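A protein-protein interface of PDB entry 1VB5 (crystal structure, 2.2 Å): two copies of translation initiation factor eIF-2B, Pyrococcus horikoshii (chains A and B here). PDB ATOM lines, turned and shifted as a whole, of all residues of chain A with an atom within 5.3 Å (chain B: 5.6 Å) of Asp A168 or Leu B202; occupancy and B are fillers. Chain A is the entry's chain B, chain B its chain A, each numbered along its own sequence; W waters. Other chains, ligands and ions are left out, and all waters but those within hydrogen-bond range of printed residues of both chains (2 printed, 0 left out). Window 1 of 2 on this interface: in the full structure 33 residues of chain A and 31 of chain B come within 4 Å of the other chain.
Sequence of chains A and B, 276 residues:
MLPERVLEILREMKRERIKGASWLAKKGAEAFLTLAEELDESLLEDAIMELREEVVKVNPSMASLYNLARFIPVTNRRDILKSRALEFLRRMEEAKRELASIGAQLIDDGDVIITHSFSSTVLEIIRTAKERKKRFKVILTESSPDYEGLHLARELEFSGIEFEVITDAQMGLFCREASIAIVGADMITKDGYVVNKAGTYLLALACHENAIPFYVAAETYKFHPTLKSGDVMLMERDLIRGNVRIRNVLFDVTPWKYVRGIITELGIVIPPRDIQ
Water W1 lies within hydrogen-bond range of the side-chain carboxylate (OD2) of Asp A168 (2.8 Å), the backbone NH (N) of Ala B169 (3.0 Å) and the backbone NH (N) of Asp B168 (3.3 Å). Water W2 lies within hydrogen-bond range of the side-chain carboxylate (OD2) of Asp B168 (2.8 Å), the backbone NH (N) of Ala A169 (2.9 Å) and the backbone NH (N) of Asp A168 (3.3 Å).
Among the printed residues, merely in contact across the chains: Asp A168 with Ala B169 (3.6 Å), Ala A206 with Leu B205 (3.6 Å), Leu A202 with Ala B169 (3.7 Å), Gly A172 with Leu B202 (3.7 Å), Leu A205 with Leu B205 (3.8 Å), Ala A169 with Asp B168 (3.8 Å), Leu A205 with Ala B206 (3.8 Å), Ala A169 with Leu B202 (3.9 Å), Leu A202 with Leu B202 (3.98 Å), Ala A206 with Leu B202 (3.98 Å), Asp A168 with Leu B202 (3.98 Å) and Leu A202 with Asp B168 (3.98 Å).
The backbone NH of Ser A144 is in hydrogen-bond range of the side-chain carboxylate of Asp A168 (2.9 Å). The side-chain carboxylate (OD1) of Asp A168 sits at hydrogen-bond distance from the backbone NH (N) of Ser A143 (3.0 Å).
Of chain B, only Ala B169 and Leu B202 come within 4 Å of Asp A168. Leu B202 touches five residues of chain A. Of the printed residues of chain A, Ala B169 touches Asp A168 (3.6 Å) and Leu A202 (3.7 Å). Of the printed residues of chain A, Ala B206 touches Leu A205. The nearest residue of chain A that does not touch Leu B202 is Met A171 (4.3 Å). The nearest printed residue of chain B that does not touch Leu A202 is Ala B206 (4.02 Å).
The backbone NH (N) of Gly B199 sits at hydrogen-bond distance from the backbone carbonyl oxygen (O) of Ala A169, 3.0 Å away.
Hydrophobic or aromatic side chains of chain B that line the printed part of chain A: Ala B169, Leu B202 and Leu B205. Among the printed residues, 13 pairs touch across the chains. Among the printed residues, no Asp or Glu carboxylate lies within 4 Å of a Lys or Arg side-chain nitrogen of the other chain.
Asp A168 touches Ala B169, and with the chains exchanged Ala A169 touches Asp B168. Ala A169 touches Leu B202, and with the chains exchanged Leu A202 touches Ala B169. Leu A202 touches its own counterpart, Leu B202. Leu A205 touches Ala B206, and with the chains exchanged Ala A206 touches Leu B205. 6 positions are printed for both chains.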
ATOM      1  N   HIS A 116      35.458  15.724  -6.373  1.00  0.00           N
ATOM      2  CA  HIS A 116      36.001  16.911  -5.719  1.00  0.00           C
ATOM      3  C   HIS A 116      37.347  16.554  -5.095  1.00  0.00           C
ATOM      4  O   HIS A 116      37.539  15.433  -4.630  1.00  0.00           O
ATOM      5  CB  HIS A 116      35.001  17.392  -4.649  1.00  0.00           C
ATOM      6  CG  HIS A 116      35.490  18.532  -3.808  1.00  0.00           C
ATOM      7  ND1 HIS A 116      35.929  19.723  -4.345  1.00  0.00           N
ATOM      8  CD2 HIS A 116      35.589  18.667  -2.464  1.00  0.00           C
ATOM      9  CE1 HIS A 116      36.280  20.541  -3.368  1.00  0.00           C
ATOM     10  NE2 HIS A 116      36.083  19.926  -2.217  1.00  0.00           N
ATOM     11  N   THR A 141      36.668  19.501  -9.593  1.00  0.00           N
ATOM     12  CA  THR A 141      36.906  20.849  -9.103  1.00  0.00           C
ATOM     13  C   THR A 141      38.393  21.117  -8.961  1.00  0.00           C
ATOM     14  O   THR A 141      39.171  20.197  -8.723  1.00  0.00           O
ATOM     15  CB  THR A 141      36.263  21.064  -7.720  1.00  0.00           C
ATOM     16  OG1 THR A 141      36.919  20.226  -6.757  1.00  0.00           O
ATOM     17  CG2 THR A 141      34.797  20.721  -7.756  1.00  0.00           C
ATOM     18  N   GLU A 142      38.782  22.383  -9.103  1.00  0.00           N
ATOM     19  CA  GLU A 142      40.179  22.766  -8.963  1.00  0.00           C
ATOM     20  C   GLU A 142      40.598  22.564  -7.504  1.00  0.00           C
ATOM     21  O   GLU A 142      41.767  22.284  -7.221  1.00  0.00           O
ATOM     22  CB  GLU A 142      40.373  24.225  -9.384  1.00  0.00           C
ATOM     23  CG  GLU A 142      39.597  25.227  -8.558  1.00  0.00           C
ATOM     24  CD  GLU A 142      39.602  26.624  -9.178  1.00  0.00           C
ATOM     25  OE1 GLU A 142      39.029  27.555  -8.566  1.00  0.00           O
ATOM     26  OE2 GLU A 142      40.176  26.789 -10.276  1.00  0.00           O
ATOM     27  N   SER A 143      39.631  22.717  -6.595  1.00  0.00           N
ATOM     28  CA  SER A 143      39.817  22.524  -5.152  1.00  0.00           C
ATOM     29  C   SER A 143      40.674  23.552  -4.417  1.00  0.00           C
ATOM     30  O   SER A 143      41.847  23.297  -4.121  1.00  0.00           O
ATOM     31  CB  SER A 143      40.394  21.130  -4.873  1.00  0.00           C
ATOM     32  OG  SER A 143      39.643  20.125  -5.531  1.00  0.00           O
ATOM     33  N   SER A 144      40.081  24.696  -4.096  1.00  0.00           N
ATOM     34  CA  SER A 144      40.797  25.746  -3.375  1.00  0.00           C
ATOM     35  C   SER A 144      41.166  25.247  -1.981  1.00  0.00           C
ATOM     36  O   SER A 144      40.460  24.422  -1.406  1.00  0.00           O
ATOM     37  CB  SER A 144      39.918  26.994  -3.252  1.00  0.00           C
ATOM     38  OG  SER A 144      39.553  27.473  -4.532  1.00  0.00           O
ATOM     39  N   ILE A 166      36.102  22.649 -13.031  1.00  0.00           N
ATOM     40  CA  ILE A 166      35.246  23.744 -12.585  1.00  0.00           C
ATOM     41  C   ILE A 166      35.783  24.282 -11.262  1.00  0.00           C
ATOM     42  O   ILE A 166      36.705  23.703 -10.678  1.00  0.00           O
ATOM     43  CB  ILE A 166      33.769  23.279 -12.370  1.00  0.00           C
ATOM     44  CG1 ILE A 166      33.689  22.264 -11.223  1.00  0.00           C
ATOM     45  CG2 ILE A 166      33.221  22.662 -13.647  1.00  0.00           C
ATOM     46  CD1 ILE A 166      32.260  21.784 -10.906  1.00  0.00           C
ATOM     47  N   THR A 167      35.230  25.405 -10.806  1.00  0.00           N
ATOM     48  CA  THR A 167      35.639  25.979  -9.524  1.00  0.00           C
ATOM     49  C   THR A 167      34.756  25.289  -8.491  1.00  0.00           C
ATOM     50  O   THR A 167      33.719  24.731  -8.848  1.00  0.00           O
ATOM     51  CB  THR A 167      35.368  27.488  -9.467  1.00  0.00           C
ATOM     52  OG1 THR A 167      33.969  27.719  -9.640  1.00  0.00           O
ATOM     53  CG2 THR A 167      36.139  28.214 -10.569  1.00  0.00           C
ATOM     54  N   ASP A 168      35.145  25.328  -7.220  1.00  0.00           N
ATOM     55  CA  ASP A 168      34.350  24.672  -6.183  1.00  0.00           C
ATOM     56  C   ASP A 168      32.906  25.198  -6.115  1.00  0.00           C
ATOM     57  O   ASP A 168      31.959  24.426  -5.953  1.00  0.00           O
ATOM     58  CB  ASP A 168      35.014  24.836  -4.803  1.00  0.00           C
ATOM     59  CG  ASP A 168      36.478  24.367  -4.779  1.00  0.00           C
ATOM     60  OD1 ASP A 168      36.907  23.655  -5.713  1.00  0.00           O
ATOM     61  OD2 ASP A 168      37.201  24.701  -3.810  1.00  0.00           O
ATOM     62  N   ALA A 169      32.738  26.510  -6.247  1.00  0.00           N
ATOM     63  CA  ALA A 169      31.412  27.113  -6.167  1.00  0.00           C
ATOM     64  C   ALA A 169      30.454  26.704  -7.288  1.00  0.00           C
ATOM     65  O   ALA A 169      29.255  26.994  -7.224  1.00  0.00           O
ATOM     66  CB  ALA A 169      31.542  28.638  -6.111  1.00  0.00           C
ATOM     67  N   GLN A 170      30.968  26.024  -8.310  1.00  0.00           N
ATOM     68  CA  GLN A 170      30.125  25.594  -9.426  1.00  0.00           C
ATOM     69  C   GLN A 170      29.586  24.162  -9.278  1.00  0.00           C
ATOM     70  O   GLN A 170      28.857  23.682 -10.145  1.00  0.00           O
ATOM     71  CB  GLN A 170      30.900  25.706 -10.742  1.00  0.00           C
ATOM     72  CG  GLN A 170      30.952  27.101 -11.356  1.00  0.00           C
ATOM     73  CD  GLN A 170      31.844  27.142 -12.590  1.00  0.00           C
ATOM     74  OE1 GLN A 170      33.057  27.315 -12.487  1.00  0.00           O
ATOM     75  NE2 GLN A 170      31.248  26.959 -13.759  1.00  0.00           N
ATOM     76  N   MET A 171      29.939  23.491  -8.183  1.00  0.00           N
ATOM     77  CA  MET A 171      29.499  22.112  -7.955  1.00  0.00           C
ATOM     78  C   MET A 171      27.991  21.919  -8.067  1.00  0.00           C
ATOM     79  O   MET A 171      27.533  20.885  -8.553  1.00  0.00           O
ATOM     80  CB  MET A 171      29.987  21.610  -6.592  1.00  0.00           C
ATOM     81  CG  MET A 171      31.490  21.443  -6.524  1.00  0.00           C
ATOM     82  SD  MET A 171      32.052  20.579  -5.044  1.00  0.00           S
ATOM     83  CE  MET A 171      31.650  21.779  -3.744  1.00  0.00           C
ATOM     84  N   GLY A 172      27.223  22.907  -7.617  1.00  0.00           N
ATOM     85  CA  GLY A 172      25.774  22.811  -7.699  1.00  0.00           C
ATOM     86  C   GLY A 172      25.262  22.897  -9.125  1.00  0.00           C
ATOM     87  O   GLY A 172      24.280  22.247  -9.482  1.00  0.00           O
ATOM     88  N   LEU A 202      28.850  20.021   0.521  1.00  0.00           N
ATOM     89  CA  LEU A 202      28.036  20.798  -0.416  1.00  0.00           C
ATOM     90  C   LEU A 202      27.753  19.985  -1.670  1.00  0.00           C
ATOM     91  O   LEU A 202      26.653  20.036  -2.219  1.00  0.00           O
ATOM     92  CB  LEU A 202      28.745  22.101  -0.798  1.00  0.00           C
ATOM     93  CG  LEU A 202      29.154  22.984   0.383  1.00  0.00           C
ATOM     94  CD1 LEU A 202      29.884  24.229  -0.119  1.00  0.00           C
ATOM     95  CD2 LEU A 202      27.915  23.358   1.181  1.00  0.00           C
ATOM     96  N   LEU A 205      25.063  17.596  -0.795  1.00  0.00           N
ATOM     97  CA  LEU A 205      23.737  18.211  -0.718  1.00  0.00           C
ATOM     98  C   LEU A 205      23.144  18.457  -2.097  1.00  0.00           C
ATOM     99  O   LEU A 205      21.982  18.147  -2.339  1.00  0.00           O
ATOM    100  CB  LEU A 205      23.799  19.536   0.055  1.00  0.00           C
ATOM    101  CG  LEU A 205      24.147  19.449   1.548  1.00  0.00           C
ATOM    102  CD1 LEU A 205      24.259  20.859   2.139  1.00  0.00           C
ATOM    103  CD2 LEU A 205      23.078  18.648   2.277  1.00  0.00           C
ATOM    104  N   ALA A 206      23.946  19.004  -3.006  1.00  0.00           N
ATOM    105  CA  ALA A 206      23.467  19.307  -4.354  1.00  0.00           C
ATOM    106  C   ALA A 206      23.083  18.062  -5.138  1.00  0.00           C
ATOM    107  O   ALA A 206      22.073  18.034  -5.847  1.00  0.00           O
ATOM    108  CB  ALA A 206      24.534  20.087  -5.122  1.00  0.00           C
ATOM    109  N   ASP B 168      35.117  29.409  -0.805  1.00  0.00           N
ATOM    110  CA  ASP B 168      33.768  29.040  -1.200  1.00  0.00           C
ATOM    111  C   ASP B 168      33.368  27.642  -0.717  1.00  0.00           C
ATOM    112  O   ASP B 168      32.242  27.431  -0.244  1.00  0.00           O
ATOM    113  CB  ASP B 168      33.631  29.130  -2.728  1.00  0.00           C
ATOM    114  CG  ASP B 168      34.005  30.510  -3.276  1.00  0.00           C
ATOM    115  OD1 ASP B 168      33.977  31.492  -2.498  1.00  0.00           O
ATOM    116  OD2 ASP B 168      34.310  30.621  -4.487  1.00  0.00           O
ATOM    117  N   ALA B 169      34.296  26.697  -0.825  1.00  0.00           N
ATOM    118  CA  ALA B 169      34.054  25.311  -0.428  1.00  0.00           C
ATOM    119  C   ALA B 169      33.730  25.142   1.053  1.00  0.00           C
ATOM    120  O   ALA B 169      33.186  24.121   1.455  1.00  0.00           O
ATOM    121  CB  ALA B 169      35.277  24.447  -0.796  1.00  0.00           C
ATOM    122  N   MET B 171      31.555  26.967   2.847  1.00  0.00           N
ATOM    123  CA  MET B 171      30.259  27.534   3.230  1.00  0.00           C
ATOM    124  C   MET B 171      29.399  26.622   4.095  1.00  0.00           C
ATOM    125  O   MET B 171      28.692  27.096   4.988  1.00  0.00           O
ATOM    126  CB  MET B 171      29.473  27.957   1.990  1.00  0.00           C
ATOM    127  CG  MET B 171      30.122  29.104   1.245  1.00  0.00           C
ATOM    128  SD  MET B 171      29.106  29.724  -0.101  1.00  0.00           S
ATOM    129  CE  MET B 171      29.371  28.452  -1.366  1.00  0.00           C
ATOM    130  N   GLY B 199      27.450  29.334  -6.751  1.00  0.00           N
ATOM    131  CA  GLY B 199      27.733  28.937  -5.384  1.00  0.00           C
ATOM    132  C   GLY B 199      26.678  29.390  -4.386  1.00  0.00           C
ATOM    133  O   GLY B 199      26.603  28.853  -3.282  1.00  0.00           O
ATOM    134  N   THR B 200      25.865  30.377  -4.760  1.00  0.00           N
ATOM    135  CA  THR B 200      24.821  30.882  -3.861  1.00  0.00           C
ATOM    136  C   THR B 200      23.841  29.765  -3.535  1.00  0.00           C
ATOM    137  O   THR B 200      23.331  29.675  -2.421  1.00  0.00           O
ATOM    138  CB  THR B 200      24.034  32.057  -4.496  1.00  0.00           C
ATOM    139  OG1 THR B 200      24.922  33.157  -4.727  1.00  0.00           O
ATOM    140  CG2 THR B 200      22.905  32.514  -3.566  1.00  0.00           C
ATOM    141  N   TYR B 201      23.590  28.916  -4.526  1.00  0.00           N
ATOM    142  CA  TYR B 201      22.684  27.781  -4.377  1.00  0.00           C
ATOM    143  C   TYR B 201      23.188  26.831  -3.287  1.00  0.00           C
ATOM    144  O   TYR B 201      22.406  26.324  -2.481  1.00  0.00           O
ATOM    145  CB  TYR B 201      22.586  27.036  -5.713  1.00  0.00           C
ATOM    146  CG  TYR B 201      21.857  25.707  -5.669  1.00  0.00           C
ATOM    147  CD1 TYR B 201      20.507  25.634  -5.318  1.00  0.00           C
ATOM    148  CD2 TYR B 201      22.515  24.521  -6.005  1.00  0.00           C
ATOM    149  CE1 TYR B 201      19.827  24.411  -5.303  1.00  0.00           C
ATOM    150  CE2 TYR B 201      21.848  23.293  -5.995  1.00  0.00           C
ATOM    151  CZ  TYR B 201      20.510  23.249  -5.645  1.00  0.00           C
ATOM    152  OH  TYR B 201      19.854  22.047  -5.629  1.00  0.00           O
ATOM    153  N   LEU B 202      24.499  26.606  -3.266  1.00  0.00           N
ATOM    154  CA  LEU B 202      25.114  25.713  -2.283  1.00  0.00           C
ATOM    155  C   LEU B 202      24.964  26.273  -0.871  1.00  0.00           C
ATOM    156  O   LEU B 202      24.662  25.536   0.063  1.00  0.00           O
ATOM    157  CB  LEU B 202      26.602  25.504  -2.606  1.00  0.00           C
ATOM    158  CG  LEU B 202      26.917  24.895  -3.982  1.00  0.00           C
ATOM    159  CD1 LEU B 202      28.426  24.805  -4.167  1.00  0.00           C
ATOM    160  CD2 LEU B 202      26.274  23.515  -4.106  1.00  0.00           C
ATOM    161  N   LEU B 203      25.181  27.577  -0.718  1.00  0.00           N
ATOM    162  CA  LEU B 203      25.039  28.204   0.590  1.00  0.00           C
ATOM    163  C   LEU B 203      23.587  28.050   1.024  1.00  0.00           C
ATOM    164  O   LEU B 203      23.305  27.748   2.180  1.00  0.00           O
ATOM    165  CB  LEU B 203      25.420  29.689   0.518  1.00  0.00           C
ATOM    166  CG  LEU B 203      25.271  30.544   1.784  1.00  0.00           C
ATOM    167  CD1 LEU B 203      26.177  30.030   2.892  1.00  0.00           C
ATOM    168  CD2 LEU B 203      25.637  31.982   1.458  1.00  0.00           C
ATOM    169  N   ALA B 204      22.663  28.239   0.087  1.00  0.00           N
ATOM    170  CA  ALA B 204      21.241  28.117   0.396  1.00  0.00           C
ATOM    171  C   ALA B 204      20.911  26.707   0.904  1.00  0.00           C
ATOM    172  O   ALA B 204      20.153  26.542   1.864  1.00  0.00           O
ATOM    173  CB  ALA B 204      20.403  28.445  -0.838  1.00  0.00           C
ATOM    174  N   LEU B 205      21.480  25.691   0.265  1.00  0.00           N
ATOM    175  CA  LEU B 205      21.217  24.319   0.686  1.00  0.00           C
ATOM    176  C   LEU B 205      21.732  24.071   2.090  1.00  0.00           C
ATOM    177  O   LEU B 205      21.029  23.505   2.922  1.00  0.00           O
ATOM    178  CB  LEU B 205      21.884  23.314  -0.255  1.00  0.00           C
ATOM    179  CG  LEU B 205      21.349  23.201  -1.676  1.00  0.00           C
ATOM    180  CD1 LEU B 205      22.064  22.040  -2.367  1.00  0.00           C
ATOM    181  CD2 LEU B 205      19.854  22.969  -1.655  1.00  0.00           C
ATOM    182  N   ALA B 206      22.964  24.502   2.341  1.00  0.00           N
ATOM    183  CA  ALA B 206      23.604  24.312   3.631  1.00  0.00           C
ATOM    184  C   ALA B 206      22.845  25.025   4.739  1.00  0.00           C
ATOM    185  O   ALA B 206      22.602  24.474   5.810  1.00  0.00           O
ATOM    186  CB  ALA B 206      25.038  24.820   3.573  1.00  0.00           C
ATOM    187  N   CYS B 207      22.474  26.265   4.477  1.00  0.00           N
ATOM    188  CA  CYS B 207      21.751  27.042   5.466  1.00  0.00           C
ATOM    189  C   CYS B 207      20.364  26.440   5.778  1.00  0.00           C
ATOM    190  O   CYS B 207      19.892  26.517   6.913  1.00  0.00           O
ATOM    191  CB  CYS B 207      21.668  28.487   4.983  1.00  0.00           C
ATOM    192  SG  CYS B 207      23.174  29.510   5.236  1.00  0.00           S
ATOM    193  N   ASP B 252      24.361  31.173 -10.959  1.00  0.00           N
ATOM    194  CA  ASP B 252      23.549  30.003 -10.638  1.00  0.00           C
ATOM    195  C   ASP B 252      22.122  30.432 -10.305  1.00  0.00           C
ATOM    196  O   ASP B 252      21.810  31.627 -10.240  1.00  0.00           O
ATOM    197  CB  ASP B 252      24.113  29.302  -9.403  1.00  0.00           C
ATOM    198  CG  ASP B 252      23.588  29.916  -8.099  1.00  0.00           C
ATOM    199  OD1 ASP B 252      22.539  29.459  -7.585  1.00  0.00           O
ATOM    200  OD2 ASP B 252      24.209  30.877  -7.606  1.00  0.00           O
HETATM  201  O   HOH W   1      36.612  27.141  -2.647  1.00  0.00           O
HETATM  202  O   HOH W   2      34.961  28.302  -5.887  1.00  0.00           O
